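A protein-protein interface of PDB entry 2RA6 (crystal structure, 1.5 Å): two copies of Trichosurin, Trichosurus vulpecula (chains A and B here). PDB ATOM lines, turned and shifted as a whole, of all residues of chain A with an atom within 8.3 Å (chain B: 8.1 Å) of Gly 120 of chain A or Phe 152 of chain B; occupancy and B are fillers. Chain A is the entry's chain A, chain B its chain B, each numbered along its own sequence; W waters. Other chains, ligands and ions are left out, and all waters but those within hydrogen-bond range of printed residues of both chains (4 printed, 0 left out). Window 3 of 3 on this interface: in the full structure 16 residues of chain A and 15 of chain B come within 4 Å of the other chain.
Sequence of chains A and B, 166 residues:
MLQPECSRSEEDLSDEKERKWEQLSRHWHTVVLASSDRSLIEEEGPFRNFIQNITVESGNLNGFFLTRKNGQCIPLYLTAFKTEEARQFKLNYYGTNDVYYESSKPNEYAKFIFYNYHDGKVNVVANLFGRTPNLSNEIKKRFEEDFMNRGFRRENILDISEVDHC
OG1 of Thr 96 of chain A lies within hydrogen-bond range of O of Arg 150 of chain B (3.0 Å). The side-chain carboxylate of Asp 98 of chain A lies within salt-bridge range of the guanidinium group of Arg 150 of chain B.
N of Tyr 117 of chain A is in hydrogen-bond range of O of Thr 96 of chain A (2.9 Å). The side-chain carboxylate of Asp 98 of chain A sits at hydrogen-bond distance from the side-chain hydroxyl of Tyr 117 of chain A (2.6 Å). The side-chain amide oxygen of Asn 123 of chain B is in hydrogen-bond range of the side-chain hydroxyl of Ser 36 of chain B (2.7 Å). The backbone NH (N) of Val 124 of chain B lies within hydrogen-bond range of the side-chain hydroxyl (OG) of Ser 36 of chain B, 2.9 Å away. O of Ser 36 of chain B lies within hydrogen-bond range of ND2 of Asn 156 of chain B, 3.4 Å away. The backbone carbonyl oxygen of Glu 145 of chain B lies close to the side-chain amide nitrogen of Asn 149 of chain B.
Among the printed residues, merely in contact across the chains: Tyr 117 of chain A with Arg 150 of chain B (3.3 Å), Val 122 of chain A with Val 122 of chain B (3.5 Å), Gly 120 of chain A with Phe 152 of chain B (3.6 Å), Tyr 117 of chain A with Phe 152 of chain B (3.6 Å), Val 122 of chain A with Ser 36 of chain B (3.8 Å), Val 122 of chain A with Phe 152 of chain B (3.9 Å) and Thr 96 of chain A with Asn 149 of chain B (3.9 Å).
Printed residues of chain B within 4 Å of Thr 96 of chain A: Asn 149 and Arg 150. Printed residues of chain B within 4 Å of Tyr 117 of chain A: Arg 150 (3.3 Å) and Phe 152 (3.6 Å). Of chain B, only Phe 152 (3.6 Å) comes within 4 Å of Gly 120 of chain A. Of the printed residues of chain A, Val 122 of chain B touches Val 122. Asn 123 of chain B touches none of the printed residues of chain A. Phe 147 of chain B touches none of the printed residues of chain A. Of the printed residues of chain A, Asn 149 of chain B touches Thr 96. No residue of chain A comes within 4 Å of Gly 151 of chain B. Phe 152 of chain B touches just these residues of chain A: Tyr 117 (3.6 Å), Gly 120 (3.6 Å) and Val 122 (3.9 Å). The nearest residue of chain B that does not touch Gly 120 of chain A is Gly 151 of chain B (4.1 Å). The nearest residue of chain A that does not touch Phe 152 of chain B is Lys 121 of chain A (4.8 Å). The nearest printed residue of chain A that does not touch Asn 149 of chain B is Tyr 117 of chain A (7.1 Å).
Of the 11 printed residues of chain A, 5 touch a printed residue of chain B. Printed residues of chain A that touch a printed residue of chain B: Thr 96, Asp 98, Tyr 117, Gly 120 and Val 122. Hydrophobic or aromatic side chains of chain A within 4 Å of the printed part of chain B: Tyr 117 and Val 122. Of the 23 printed residues of chain B, 5 touch a printed residue of chain A. Hydrophobic or aromatic side chains of chain B within 4 Å of the printed part of chain A: Val 122 and Phe 152.
Val 122 of chain B touches its own counterpart, Val 122 of chain A. Positions printed for both chains: 121, 122 and 123. Of the 9 pairs that touch across the chains among the printed residues, 1 has its exchanged pair printed and touching as well.
Water W4 lies within hydrogen-bond range of O of Ser 36 of chain B (2.7 Å) and O of Gly 120 of chain A (2.8 Å). Water W1 lies within hydrogen-bond range of the backbone carbonyl oxygen of Tyr 117 of chain A and the backbone carbonyl oxygen of Arg 150 of chain B. Water W2 lies within hydrogen-bond range of the backbone carbonyl oxygen (O) of Val 122 of chain B (2.7 Å) and the backbone NH (N) of Val 122 of chain A (2.9 Å). Water W3 lies within hydrogen-bond range of N of Val 122 of chain B (2.8 Å), O of Val 122 of chain A (3.0 Å) and ND2 of Asn 123 of chain A (3.3 Å).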
ATOM      1  N   GLY A  95     -17.244  16.572  26.769  1.00  0.00           N
ATOM      2  CA  GLY A  95     -17.428  18.006  26.865  1.00  0.00           C
ATOM      3  C   GLY A  95     -17.222  18.395  28.314  1.00  0.00           C
ATOM      4  O   GLY A  95     -16.309  17.893  28.974  1.00  0.00           O
ATOM      5  N   THR A  96     -18.060  19.294  28.817  1.00  0.00           N
ATOM      6  CA  THR A  96     -17.960  19.716  30.206  1.00  0.00           C
ATOM      7  C   THR A  96     -19.288  19.414  30.879  1.00  0.00           C
ATOM      8  O   THR A  96     -20.317  19.321  30.211  1.00  0.00           O
ATOM      9  CB  THR A  96     -17.650  21.223  30.321  1.00  0.00           C
ATOM     10  OG1 THR A  96     -18.702  21.980  29.716  1.00  0.00           O
ATOM     11  CG2 THR A  96     -16.336  21.545  29.622  1.00  0.00           C
ATOM     12  N   ASP A  98     -21.737  20.156  34.597  1.00  0.00           N
ATOM     13  CA  ASP A  98     -21.991  20.735  35.905  1.00  0.00           C
ATOM     14  C   ASP A  98     -22.747  19.591  36.577  1.00  0.00           C
ATOM     15  O   ASP A  98     -23.803  19.172  36.103  1.00  0.00           O
ATOM     16  CB  ASP A  98     -22.851  21.989  35.772  1.00  0.00           C
ATOM     17  CG  ASP A  98     -22.018  23.219  35.442  1.00  0.00           C
ATOM     18  OD1 ASP A  98     -22.517  24.129  34.755  1.00  0.00           O
ATOM     19  OD2 ASP A  98     -20.849  23.283  35.891  1.00  0.00           O
ATOM     20  N   ASN A 116     -24.797  18.394  30.806  1.00  0.00           N
ATOM     21  CA  ASN A 116     -23.722  18.215  29.847  1.00  0.00           C
ATOM     22  C   ASN A 116     -23.726  19.244  28.736  1.00  0.00           C
ATOM     23  O   ASN A 116     -24.771  19.560  28.176  1.00  0.00           O
ATOM     24  CB  ASN A 116     -23.802  16.803  29.259  1.00  0.00           C
ATOM     25  CG  ASN A 116     -22.823  16.583  28.122  1.00  0.00           C
ATOM     26  OD1 ASN A 116     -23.210  16.588  26.955  1.00  0.00           O
ATOM     27  ND2 ASN A 116     -21.547  16.395  28.457  1.00  0.00           N
ATOM     28  N   TYR A 117     -22.547  19.782  28.446  1.00  0.00           N
ATOM     29  CA  TYR A 117     -22.402  20.757  27.375  1.00  0.00           C
ATOM     30  C   TYR A 117     -21.467  20.122  26.356  1.00  0.00           C
ATOM     31  O   TYR A 117     -20.281  19.921  26.624  1.00  0.00           O
ATOM     32  CB  TYR A 117     -21.801  22.066  27.900  1.00  0.00           C
ATOM     33  CG  TYR A 117     -22.431  22.568  29.176  1.00  0.00           C
ATOM     34  CD1 TYR A 117     -21.866  22.269  30.412  1.00  0.00           C
ATOM     35  CD2 TYR A 117     -23.601  23.326  29.152  1.00  0.00           C
ATOM     36  CE1 TYR A 117     -22.446  22.710  31.596  1.00  0.00           C
ATOM     37  CE2 TYR A 117     -24.193  23.770  30.336  1.00  0.00           C
ATOM     38  CZ  TYR A 117     -23.605  23.457  31.552  1.00  0.00           C
ATOM     39  OH  TYR A 117     -24.167  23.889  32.733  1.00  0.00           O
ATOM     40  N   HIS A 118     -22.015  19.781  25.195  1.00  0.00           N
ATOM     41  CA  HIS A 118     -21.235  19.150  24.134  1.00  0.00           C
ATOM     42  C   HIS A 118     -21.526  19.832  22.808  1.00  0.00           C
ATOM     43  O   HIS A 118     -22.669  19.852  22.362  1.00  0.00           O
ATOM     44  CB  HIS A 118     -21.597  17.666  24.024  1.00  0.00           C
ATOM     45  CG  HIS A 118     -20.781  16.918  23.014  1.00  0.00           C
ATOM     46  ND1 HIS A 118     -19.476  16.546  23.245  1.00  0.00           N
ATOM     47  CD2 HIS A 118     -21.081  16.489  21.766  1.00  0.00           C
ATOM     48  CE1 HIS A 118     -19.004  15.917  22.181  1.00  0.00           C
ATOM     49  NE2 HIS A 118     -19.961  15.871  21.269  1.00  0.00           N
ATOM     50  N   ASP A 119     -20.494  20.388  22.183  1.00  0.00           N
ATOM     51  CA  ASP A 119     -20.658  21.068  20.902  1.00  0.00           C
ATOM     52  C   ASP A 119     -21.728  22.153  20.968  1.00  0.00           C
ATOM     53  O   ASP A 119     -22.521  22.310  20.041  1.00  0.00           O
ATOM     54  CB  ASP A 119     -21.019  20.054  19.813  1.00  0.00           C
ATOM     55  CG  ASP A 119     -19.873  19.112  19.488  1.00  0.00           C
ATOM     56  OD1 ASP A 119     -20.080  18.183  18.676  1.00  0.00           O
ATOM     57  OD2 ASP A 119     -18.767  19.302  20.036  1.00  0.00           O
ATOM     58  N   GLY A 120     -21.749  22.888  22.077  1.00  0.00           N
ATOM     59  CA  GLY A 120     -22.715  23.963  22.247  1.00  0.00           C
ATOM     60  C   GLY A 120     -24.134  23.503  22.544  1.00  0.00           C
ATOM     61  O   GLY A 120     -25.050  24.323  22.625  1.00  0.00           O
ATOM     62  N   LYS A 121     -24.313  22.194  22.701  1.00  0.00           N
ATOM     63  CA  LYS A 121     -25.619  21.602  22.993  1.00  0.00           C
ATOM     64  C   LYS A 121     -25.696  21.195  24.461  1.00  0.00           C
ATOM     65  O   LYS A 121     -24.751  20.621  24.997  1.00  0.00           O
ATOM     66  CB  LYS A 121     -25.847  20.361  22.124  1.00  0.00           C
ATOM     67  CG  LYS A 121     -27.157  19.641  22.406  1.00  0.00           C
ATOM     68  CD  LYS A 121     -27.229  18.267  21.746  1.00  0.00           C
ATOM     69  CE  LYS A 121     -27.247  18.346  20.229  1.00  0.00           C
ATOM     70  NZ  LYS A 121     -27.399  16.984  19.627  1.00  0.00           N
ATOM     71  N   VAL A 122     -26.825  21.483  25.101  1.00  0.00           N
ATOM     72  CA  VAL A 122     -27.012  21.133  26.508  1.00  0.00           C
ATOM     73  C   VAL A 122     -27.980  19.970  26.681  1.00  0.00           C
ATOM     74  O   VAL A 122     -29.031  19.915  26.041  1.00  0.00           O
ATOM     75  CB  VAL A 122     -27.583  22.323  27.321  1.00  0.00           C
ATOM     76  CG1 VAL A 122     -27.640  21.960  28.807  1.00  0.00           C
ATOM     77  CG2 VAL A 122     -26.738  23.565  27.109  1.00  0.00           C
ATOM     78  N   ASN A 123     -27.621  19.043  27.560  1.00  0.00           N
ATOM     79  CA  ASN A 123     -28.481  17.914  27.866  1.00  0.00           C
ATOM     80  C   ASN A 123     -28.397  17.629  29.343  1.00  0.00           C
ATOM     81  O   ASN A 123     -27.412  17.975  29.994  1.00  0.00           O
ATOM     82  CB  ASN A 123     -28.077  16.658  27.097  1.00  0.00           C
ATOM     83  CG  ASN A 123     -28.604  16.657  25.682  1.00  0.00           C
ATOM     84  OD1 ASN A 123     -27.840  16.785  24.724  1.00  0.00           O
ATOM     85  ND2 ASN A 123     -29.922  16.517  25.542  1.00  0.00           N
ATOM     86  N   ALA B  34     -26.669  35.459  29.167  1.00  0.00           N
ATOM     87  CA  ALA B  34     -25.890  34.529  28.359  1.00  0.00           C
ATOM     88  C   ALA B  34     -26.738  33.292  28.191  1.00  0.00           C
ATOM     89  O   ALA B  34     -27.495  32.919  29.085  1.00  0.00           O
ATOM     90  CB  ALA B  34     -24.575  34.190  29.048  1.00  0.00           C
ATOM     91  N   SER B  35     -26.647  32.664  27.027  1.00  0.00           N
ATOM     92  CA  SER B  35     -27.451  31.480  26.792  1.00  0.00           C
ATOM     93  C   SER B  35     -26.860  30.570  25.748  1.00  0.00           C
ATOM     94  O   SER B  35     -26.105  31.007  24.882  1.00  0.00           O
ATOM     95  CB  SER B  35     -28.860  31.874  26.349  1.00  0.00           C
ATOM     96  OG  SER B  35     -29.674  30.726  26.128  1.00  0.00           O
ATOM     97  N   SER B  36     -27.227  29.299  25.847  1.00  0.00           N
ATOM     98  CA  SER B  36     -26.787  28.298  24.894  1.00  0.00           C
ATOM     99  C   SER B  36     -27.493  28.570  23.563  1.00  0.00           C
ATOM    100  O   SER B  36     -27.019  28.153  22.505  1.00  0.00           O
ATOM    101  CB  SER B  36     -27.123  26.897  25.420  1.00  0.00           C
ATOM    102  OG  SER B  36     -28.464  26.822  25.859  1.00  0.00           O
ATOM    103  N   ASP B  37     -28.622  29.272  23.623  1.00  0.00           N
ATOM    104  CA  ASP B  37     -29.380  29.637  22.425  1.00  0.00           C
ATOM    105  C   ASP B  37     -29.572  31.149  22.466  1.00  0.00           C
ATOM    106  O   ASP B  37     -30.429  31.655  23.198  1.00  0.00           O
ATOM    107  CB  ASP B  37     -30.744  28.945  22.413  1.00  0.00           C
ATOM    108  CG  ASP B  37     -31.474  29.119  21.088  1.00  0.00           C
ATOM    109  OD1 ASP B  37     -31.391  30.215  20.501  1.00  0.00           O
ATOM    110  OD2 ASP B  37     -32.133  28.155  20.650  1.00  0.00           O
ATOM    111  N   LYS B 121     -36.415  19.915  24.979  1.00  0.00           N
ATOM    112  CA  LYS B 121     -35.062  20.402  24.738  1.00  0.00           C
ATOM    113  C   LYS B 121     -34.558  21.178  25.944  1.00  0.00           C
ATOM    114  O   LYS B 121     -35.319  21.902  26.587  1.00  0.00           O
ATOM    115  CB  LYS B 121     -35.017  21.313  23.509  1.00  0.00           C
ATOM    116  CG  LYS B 121     -33.608  21.776  23.167  1.00  0.00           C
ATOM    117  CD  LYS B 121     -33.584  22.696  21.959  1.00  0.00           C
ATOM    118  CE  LYS B 121     -32.170  23.176  21.676  1.00  0.00           C
ATOM    119  NZ  LYS B 121     -32.111  24.109  20.514  1.00  0.00           N
ATOM    120  N   VAL B 122     -33.275  21.027  26.243  1.00  0.00           N
ATOM    121  CA  VAL B 122     -32.681  21.727  27.371  1.00  0.00           C
ATOM    122  C   VAL B 122     -31.819  22.890  26.912  1.00  0.00           C
ATOM    123  O   VAL B 122     -31.052  22.779  25.947  1.00  0.00           O
ATOM    124  CB  VAL B 122     -31.776  20.796  28.208  1.00  0.00           C
ATOM    125  CG1 VAL B 122     -31.294  21.527  29.449  1.00  0.00           C
ATOM    126  CG2 VAL B 122     -32.516  19.527  28.576  1.00  0.00           C
ATOM    127  N   ASN B 123     -31.960  24.018  27.594  1.00  0.00           N
ATOM    128  CA  ASN B 123     -31.135  25.175  27.297  1.00  0.00           C
ATOM    129  C   ASN B 123     -30.706  25.783  28.600  1.00  0.00           C
ATOM    130  O   ASN B 123     -31.346  25.588  29.629  1.00  0.00           O
ATOM    131  CB  ASN B 123     -31.883  26.216  26.474  1.00  0.00           C
ATOM    132  CG  ASN B 123     -31.714  25.992  24.985  1.00  0.00           C
ATOM    133  OD1 ASN B 123     -30.598  26.055  24.440  1.00  0.00           O
ATOM    134  ND2 ASN B 123     -32.811  25.728  24.319  1.00  0.00           N
ATOM    135  N   VAL B 124     -29.595  26.496  28.564  1.00  0.00           N
ATOM    136  CA  VAL B 124     -29.125  27.147  29.764  1.00  0.00           C
ATOM    137  C   VAL B 124     -29.143  28.644  29.518  1.00  0.00           C
ATOM    138  O   VAL B 124     -28.739  29.130  28.460  1.00  0.00           O
ATOM    139  CB  VAL B 124     -27.699  26.684  30.144  1.00  0.00           C
ATOM    140  CG1 VAL B 124     -26.704  27.076  29.063  1.00  0.00           C
ATOM    141  CG2 VAL B 124     -27.300  27.295  31.484  1.00  0.00           C
ATOM    142  N   VAL B 125     -29.663  29.373  30.495  1.00  0.00           N
ATOM    143  CA  VAL B 125     -29.711  30.823  30.421  1.00  0.00           C
ATOM    144  C   VAL B 125     -29.099  31.291  31.731  1.00  0.00           C
ATOM    145  O   VAL B 125     -29.563  30.921  32.809  1.00  0.00           O
ATOM    146  CB  VAL B 125     -31.163  31.363  30.312  1.00  0.00           C
ATOM    147  CG1 VAL B 125     -31.150  32.885  30.258  1.00  0.00           C
ATOM    148  CG2 VAL B 125     -31.838  30.809  29.060  1.00  0.00           C
ATOM    149  N   GLU B 144     -18.489  35.880  32.418  1.00  0.00           N
ATOM    150  CA  GLU B 144     -18.347  35.599  30.993  1.00  0.00           C
ATOM    151  C   GLU B 144     -17.388  34.450  30.697  1.00  0.00           C
ATOM    152  O   GLU B 144     -17.672  33.611  29.840  1.00  0.00           O
ATOM    153  CB  GLU B 144     -17.924  36.882  30.271  1.00  0.00           C
ATOM    154  CG  GLU B 144     -19.096  37.846  30.109  1.00  0.00           C
ATOM    155  CD  GLU B 144     -18.679  39.280  29.864  1.00  0.00           C
ATOM    156  OE1 GLU B 144     -17.637  39.500  29.215  1.00  0.00           O
ATOM    157  OE2 GLU B 144     -19.415  40.190  30.312  1.00  0.00           O
ATOM    158  N   GLU B 145     -16.266  34.396  31.408  1.00  0.00           N
ATOM    159  CA  GLU B 145     -15.302  33.325  31.195  1.00  0.00           C
ATOM    160  C   GLU B 145     -15.871  31.991  31.662  1.00  0.00           C
ATOM    161  O   GLU B 145     -15.644  30.959  31.027  1.00  0.00           O
ATOM    162  CB  GLU B 145     -13.994  33.622  31.933  1.00  0.00           C
ATOM    163  CG  GLU B 145     -13.308  34.886  31.455  1.00  0.00           C
ATOM    164  CD  GLU B 145     -11.937  35.069  32.067  1.00  0.00           C
ATOM    165  OE1 GLU B 145     -11.799  34.853  33.291  1.00  0.00           O
ATOM    166  OE2 GLU B 145     -11.003  35.440  31.327  1.00  0.00           O
ATOM    167  N   ASP B 146     -16.613  32.000  32.765  1.00  0.00           N
ATOM    168  CA  ASP B 146     -17.197  30.756  33.257  1.00  0.00           C
ATOM    169  C   ASP B 146     -18.171  30.207  32.231  1.00  0.00           C
ATOM    170  O   ASP B 146     -18.284  28.992  32.053  1.00  0.00           O
ATOM    171  CB  ASP B 146     -17.921  30.969  34.585  1.00  0.00           C
ATOM    172  CG  ASP B 146     -16.965  31.171  35.738  1.00  0.00           C
ATOM    173  OD1 ASP B 146     -15.819  30.678  35.649  1.00  0.00           O
ATOM    174  OD2 ASP B 146     -17.361  31.804  36.734  1.00  0.00           O
ATOM    175  N   PHE B 147     -18.875  31.107  31.555  1.00  0.00           N
ATOM    176  CA  PHE B 147     -19.825  30.702  30.532  1.00  0.00           C
ATOM    177  C   PHE B 147     -19.077  30.113  29.336  1.00  0.00           C
ATOM    178  O   PHE B 147     -19.383  29.006  28.884  1.00  0.00           O
ATOM    179  CB  PHE B 147     -20.661  31.903  30.084  1.00  0.00           C
ATOM    180  CG  PHE B 147     -21.668  31.576  29.018  1.00  0.00           C
ATOM    181  CD1 PHE B 147     -22.778  30.790  29.304  1.00  0.00           C
ATOM    182  CD2 PHE B 147     -21.498  32.050  27.723  1.00  0.00           C
ATOM    183  CE1 PHE B 147     -23.710  30.479  28.310  1.00  0.00           C
ATOM    184  CE2 PHE B 147     -22.421  31.747  26.722  1.00  0.00           C
ATOM    185  CZ  PHE B 147     -23.528  30.959  27.020  1.00  0.00           C
ATOM    186  N   MET B 148     -18.086  30.842  28.832  1.00  0.00           N
ATOM    187  CA  MET B 148     -17.322  30.368  27.684  1.00  0.00           C
ATOM    188  C   MET B 148     -16.529  29.096  27.967  1.00  0.00           C
ATOM    189  O   MET B 148     -16.330  28.276  27.069  1.00  0.00           O
ATOM    190  CB  MET B 148     -16.392  31.475  27.180  1.00  0.00           C
ATOM    191  CG  MET B 148     -17.147  32.650  26.578  1.00  0.00           C
ATOM    192  SD  MET B 148     -16.080  33.963  25.951  1.00  0.00           S
ATOM    193  CE  MET B 148     -15.922  34.992  27.412  1.00  0.00           C
ATOM    194  N   ASN B 149     -16.087  28.925  29.210  1.00  0.00           N
ATOM    195  CA  ASN B 149     -15.316  27.742  29.580  1.00  0.00           C
ATOM    196  C   ASN B 149     -16.122  26.461  29.467  1.00  0.00           C
ATOM    197  O   ASN B 149     -15.559  25.364  29.420  1.00  0.00           O
ATOM    198  CB  ASN B 149     -14.779  27.868  31.005  1.00  0.00           C
ATOM    199  CG  ASN B 149     -13.634  28.843  31.102  1.00  0.00           C
ATOM    200  OD1 ASN B 149     -12.969  29.128  30.108  1.00  0.00           O
ATOM    201  ND2 ASN B 149     -13.384  29.350  32.300  1.00  0.00           N
ATOM    202  N   ARG B 150     -17.439  26.595  29.429  1.00  0.00           N
ATOM    203  CA  ARG B 150     -18.296  25.430  29.314  1.00  0.00           C
ATOM    204  C   ARG B 150     -18.506  25.033  27.862  1.00  0.00           C
ATOM    205  O   ARG B 150     -19.198  24.058  27.569  1.00  0.00           O
ATOM    206  CB  ARG B 150     -19.619  25.691  30.031  1.00  0.00           C
ATOM    207  CG  ARG B 150     -19.450  25.618  31.544  1.00  0.00           C
ATOM    208  CD  ARG B 150     -20.681  26.063  32.295  1.00  0.00           C
ATOM    209  NE  ARG B 150     -20.559  25.803  33.729  1.00  0.00           N
ATOM    210  CZ  ARG B 150     -19.604  26.304  34.512  1.00  0.00           C
ATOM    211  NH1 ARG B 150     -18.670  27.101  34.009  1.00  0.00           N
ATOM    212  NH2 ARG B 150     -19.583  26.005  35.805  1.00  0.00           N
ATOM    213  N   GLY B 151     -17.893  25.789  26.954  1.00  0.00           N
ATOM    214  CA  GLY B 151     -17.993  25.470  25.541  1.00  0.00           C
ATOM    215  C   GLY B 151     -18.886  26.358  24.703  1.00  0.00           C
ATOM    216  O   GLY B 151     -19.386  25.931  23.663  1.00  0.00           O
ATOM    217  N   PHE B 152     -19.090  27.598  25.135  1.00  0.00           N
ATOM    218  CA  PHE B 152     -19.933  28.515  24.384  1.00  0.00           C
ATOM    219  C   PHE B 152     -19.146  29.696  23.833  1.00  0.00           C
ATOM    220  O   PHE B 152     -18.117  30.083  24.387  1.00  0.00           O
ATOM    221  CB  PHE B 152     -21.080  29.011  25.263  1.00  0.00           C
ATOM    222  CG  PHE B 152     -21.981  27.913  25.742  1.00  0.00           C
ATOM    223  CD1 PHE B 152     -21.942  27.488  27.063  1.00  0.00           C
ATOM    224  CD2 PHE B 152     -22.850  27.279  24.858  1.00  0.00           C
ATOM    225  CE1 PHE B 152     -22.755  26.443  27.503  1.00  0.00           C
ATOM    226  CE2 PHE B 152     -23.665  26.235  25.287  1.00  0.00           C
ATOM    227  CZ  PHE B 152     -23.619  25.816  26.610  1.00  0.00           C
ATOM    228  N   ARG B 153     -19.645  30.263  22.739  1.00  0.00           N
ATOM    229  CA  ARG B 153     -18.993  31.390  22.088  1.00  0.00           C
ATOM    230  C   ARG B 153     -19.276  32.719  22.782  1.00  0.00           C
ATOM    231  O   ARG B 153     -20.317  32.900  23.413  1.00  0.00           O
ATOM    232  CB  ARG B 153     -19.432  31.472  20.623  1.00  0.00           C
ATOM    233  CG  ARG B 153     -20.927  31.665  20.424  1.00  0.00           C
ATOM    234  CD  ARG B 153     -21.258  31.941  18.962  1.00  0.00           C
ATOM    235  NE  ARG B 153     -21.035  30.780  18.103  1.00  0.00           N
ATOM    236  CZ  ARG B 153     -21.865  29.747  18.007  1.00  0.00           C
ATOM    237  NH1 ARG B 153     -22.986  29.722  18.717  1.00  0.00           N
ATOM    238  NH2 ARG B 153     -21.579  28.739  17.194  1.00  0.00           N
ATOM    239  N   ARG B 154     -18.338  33.649  22.648  1.00  0.00           N
ATOM    240  CA  ARG B 154     -18.458  34.972  23.246  1.00  0.00           C
ATOM    241  C   ARG B 154     -19.697  35.695  22.718  1.00  0.00           C
ATOM    242  O   ARG B 154     -20.303  36.513  23.415  1.00  0.00           O
ATOM    243  CB  ARG B 154     -17.197  35.785  22.935  1.00  0.00           C
ATOM    244  CG  ARG B 154     -17.180  37.195  23.492  1.00  0.00           C
ATOM    245  CD  ARG B 154     -15.924  37.927  23.035  1.00  0.00           C
ATOM    246  NE  ARG B 154     -14.703  37.260  23.483  1.00  0.00           N
ATOM    247  CZ  ARG B 154     -14.282  37.236  24.743  1.00  0.00           C
ATOM    248  NH1 ARG B 154     -14.982  37.846  25.692  1.00  0.00           N
ATOM    249  NH2 ARG B 154     -13.162  36.601  25.058  1.00  0.00           N
ATOM    250  N   GLU B 155     -20.079  35.378  21.487  1.00  0.00           N
ATOM    251  CA  GLU B 155     -21.238  35.995  20.853  1.00  0.00           C
ATOM    252  C   GLU B 155     -22.551  35.665  21.551  1.00  0.00           C
ATOM    253  O   GLU B 155     -23.551  36.350  21.346  1.00  0.00           O
ATOM    254  CB  GLU B 155     -21.317  35.561  19.388  1.00  0.00           C
ATOM    255  CG  GLU B 155     -20.129  35.994  18.553  1.00  0.00           C
ATOM    256  CD  GLU B 155     -20.092  35.306  17.201  1.00  0.00           C
ATOM    257  OE1 GLU B 155     -19.966  34.061  17.171  1.00  0.00           O
ATOM    258  OE2 GLU B 155     -20.189  36.010  16.173  1.00  0.00           O
ATOM    259  N   ASN B 156     -22.548  34.617  22.371  1.00  0.00           N
ATOM    260  CA  ASN B 156     -23.754  34.205  23.088  1.00  0.00           C
ATOM    261  C   ASN B 156     -23.909  34.916  24.424  1.00  0.00           C
ATOM    262  O   ASN B 156     -24.784  34.578  25.217  1.00  0.00           O
ATOM    263  CB  ASN B 156     -23.745  32.694  23.300  1.00  0.00           C
ATOM    264  CG  ASN B 156     -24.217  31.940  22.074  1.00  0.00           C
ATOM    265  OD1 ASN B 156     -23.867  32.288  20.947  1.00  0.00           O
ATOM    266  ND2 ASN B 156     -25.011  30.901  22.290  1.00  0.00           N
ATOM    267  N   ILE B 157     -23.048  35.898  24.660  1.00  0.00           N
ATOM    268  CA  ILE B 157     -23.089  36.689  25.882  1.00  0.00           C
ATOM    269  C   ILE B 157     -23.533  38.091  25.487  1.00  0.00           C
ATOM    270  O   ILE B 157     -22.995  38.679  24.546  1.00  0.00           O
ATOM    271  CB  ILE B 157     -21.697  36.781  26.535  1.00  0.00           C
ATOM    272  CG1 ILE B 157     -21.236  35.396  26.983  1.00  0.00           C
ATOM    273  CG2 ILE B 157     -21.740  37.753  27.713  1.00  0.00           C
ATOM    274  CD1 ILE B 157     -19.774  35.338  27.394  1.00  0.00           C
HETATM  275  O   HOH W   1     -18.421  21.693  25.761  1.00  0.00           O
HETATM  276  O   HOH W   2     -29.263  22.594  23.914  1.00  0.00           O
HETATM  277  O   HOH W   3     -31.651  19.186  24.836  1.00  0.00           O
HETATM  278  O   HOH W   4     -24.746  26.954  21.761  1.00  0.00           O
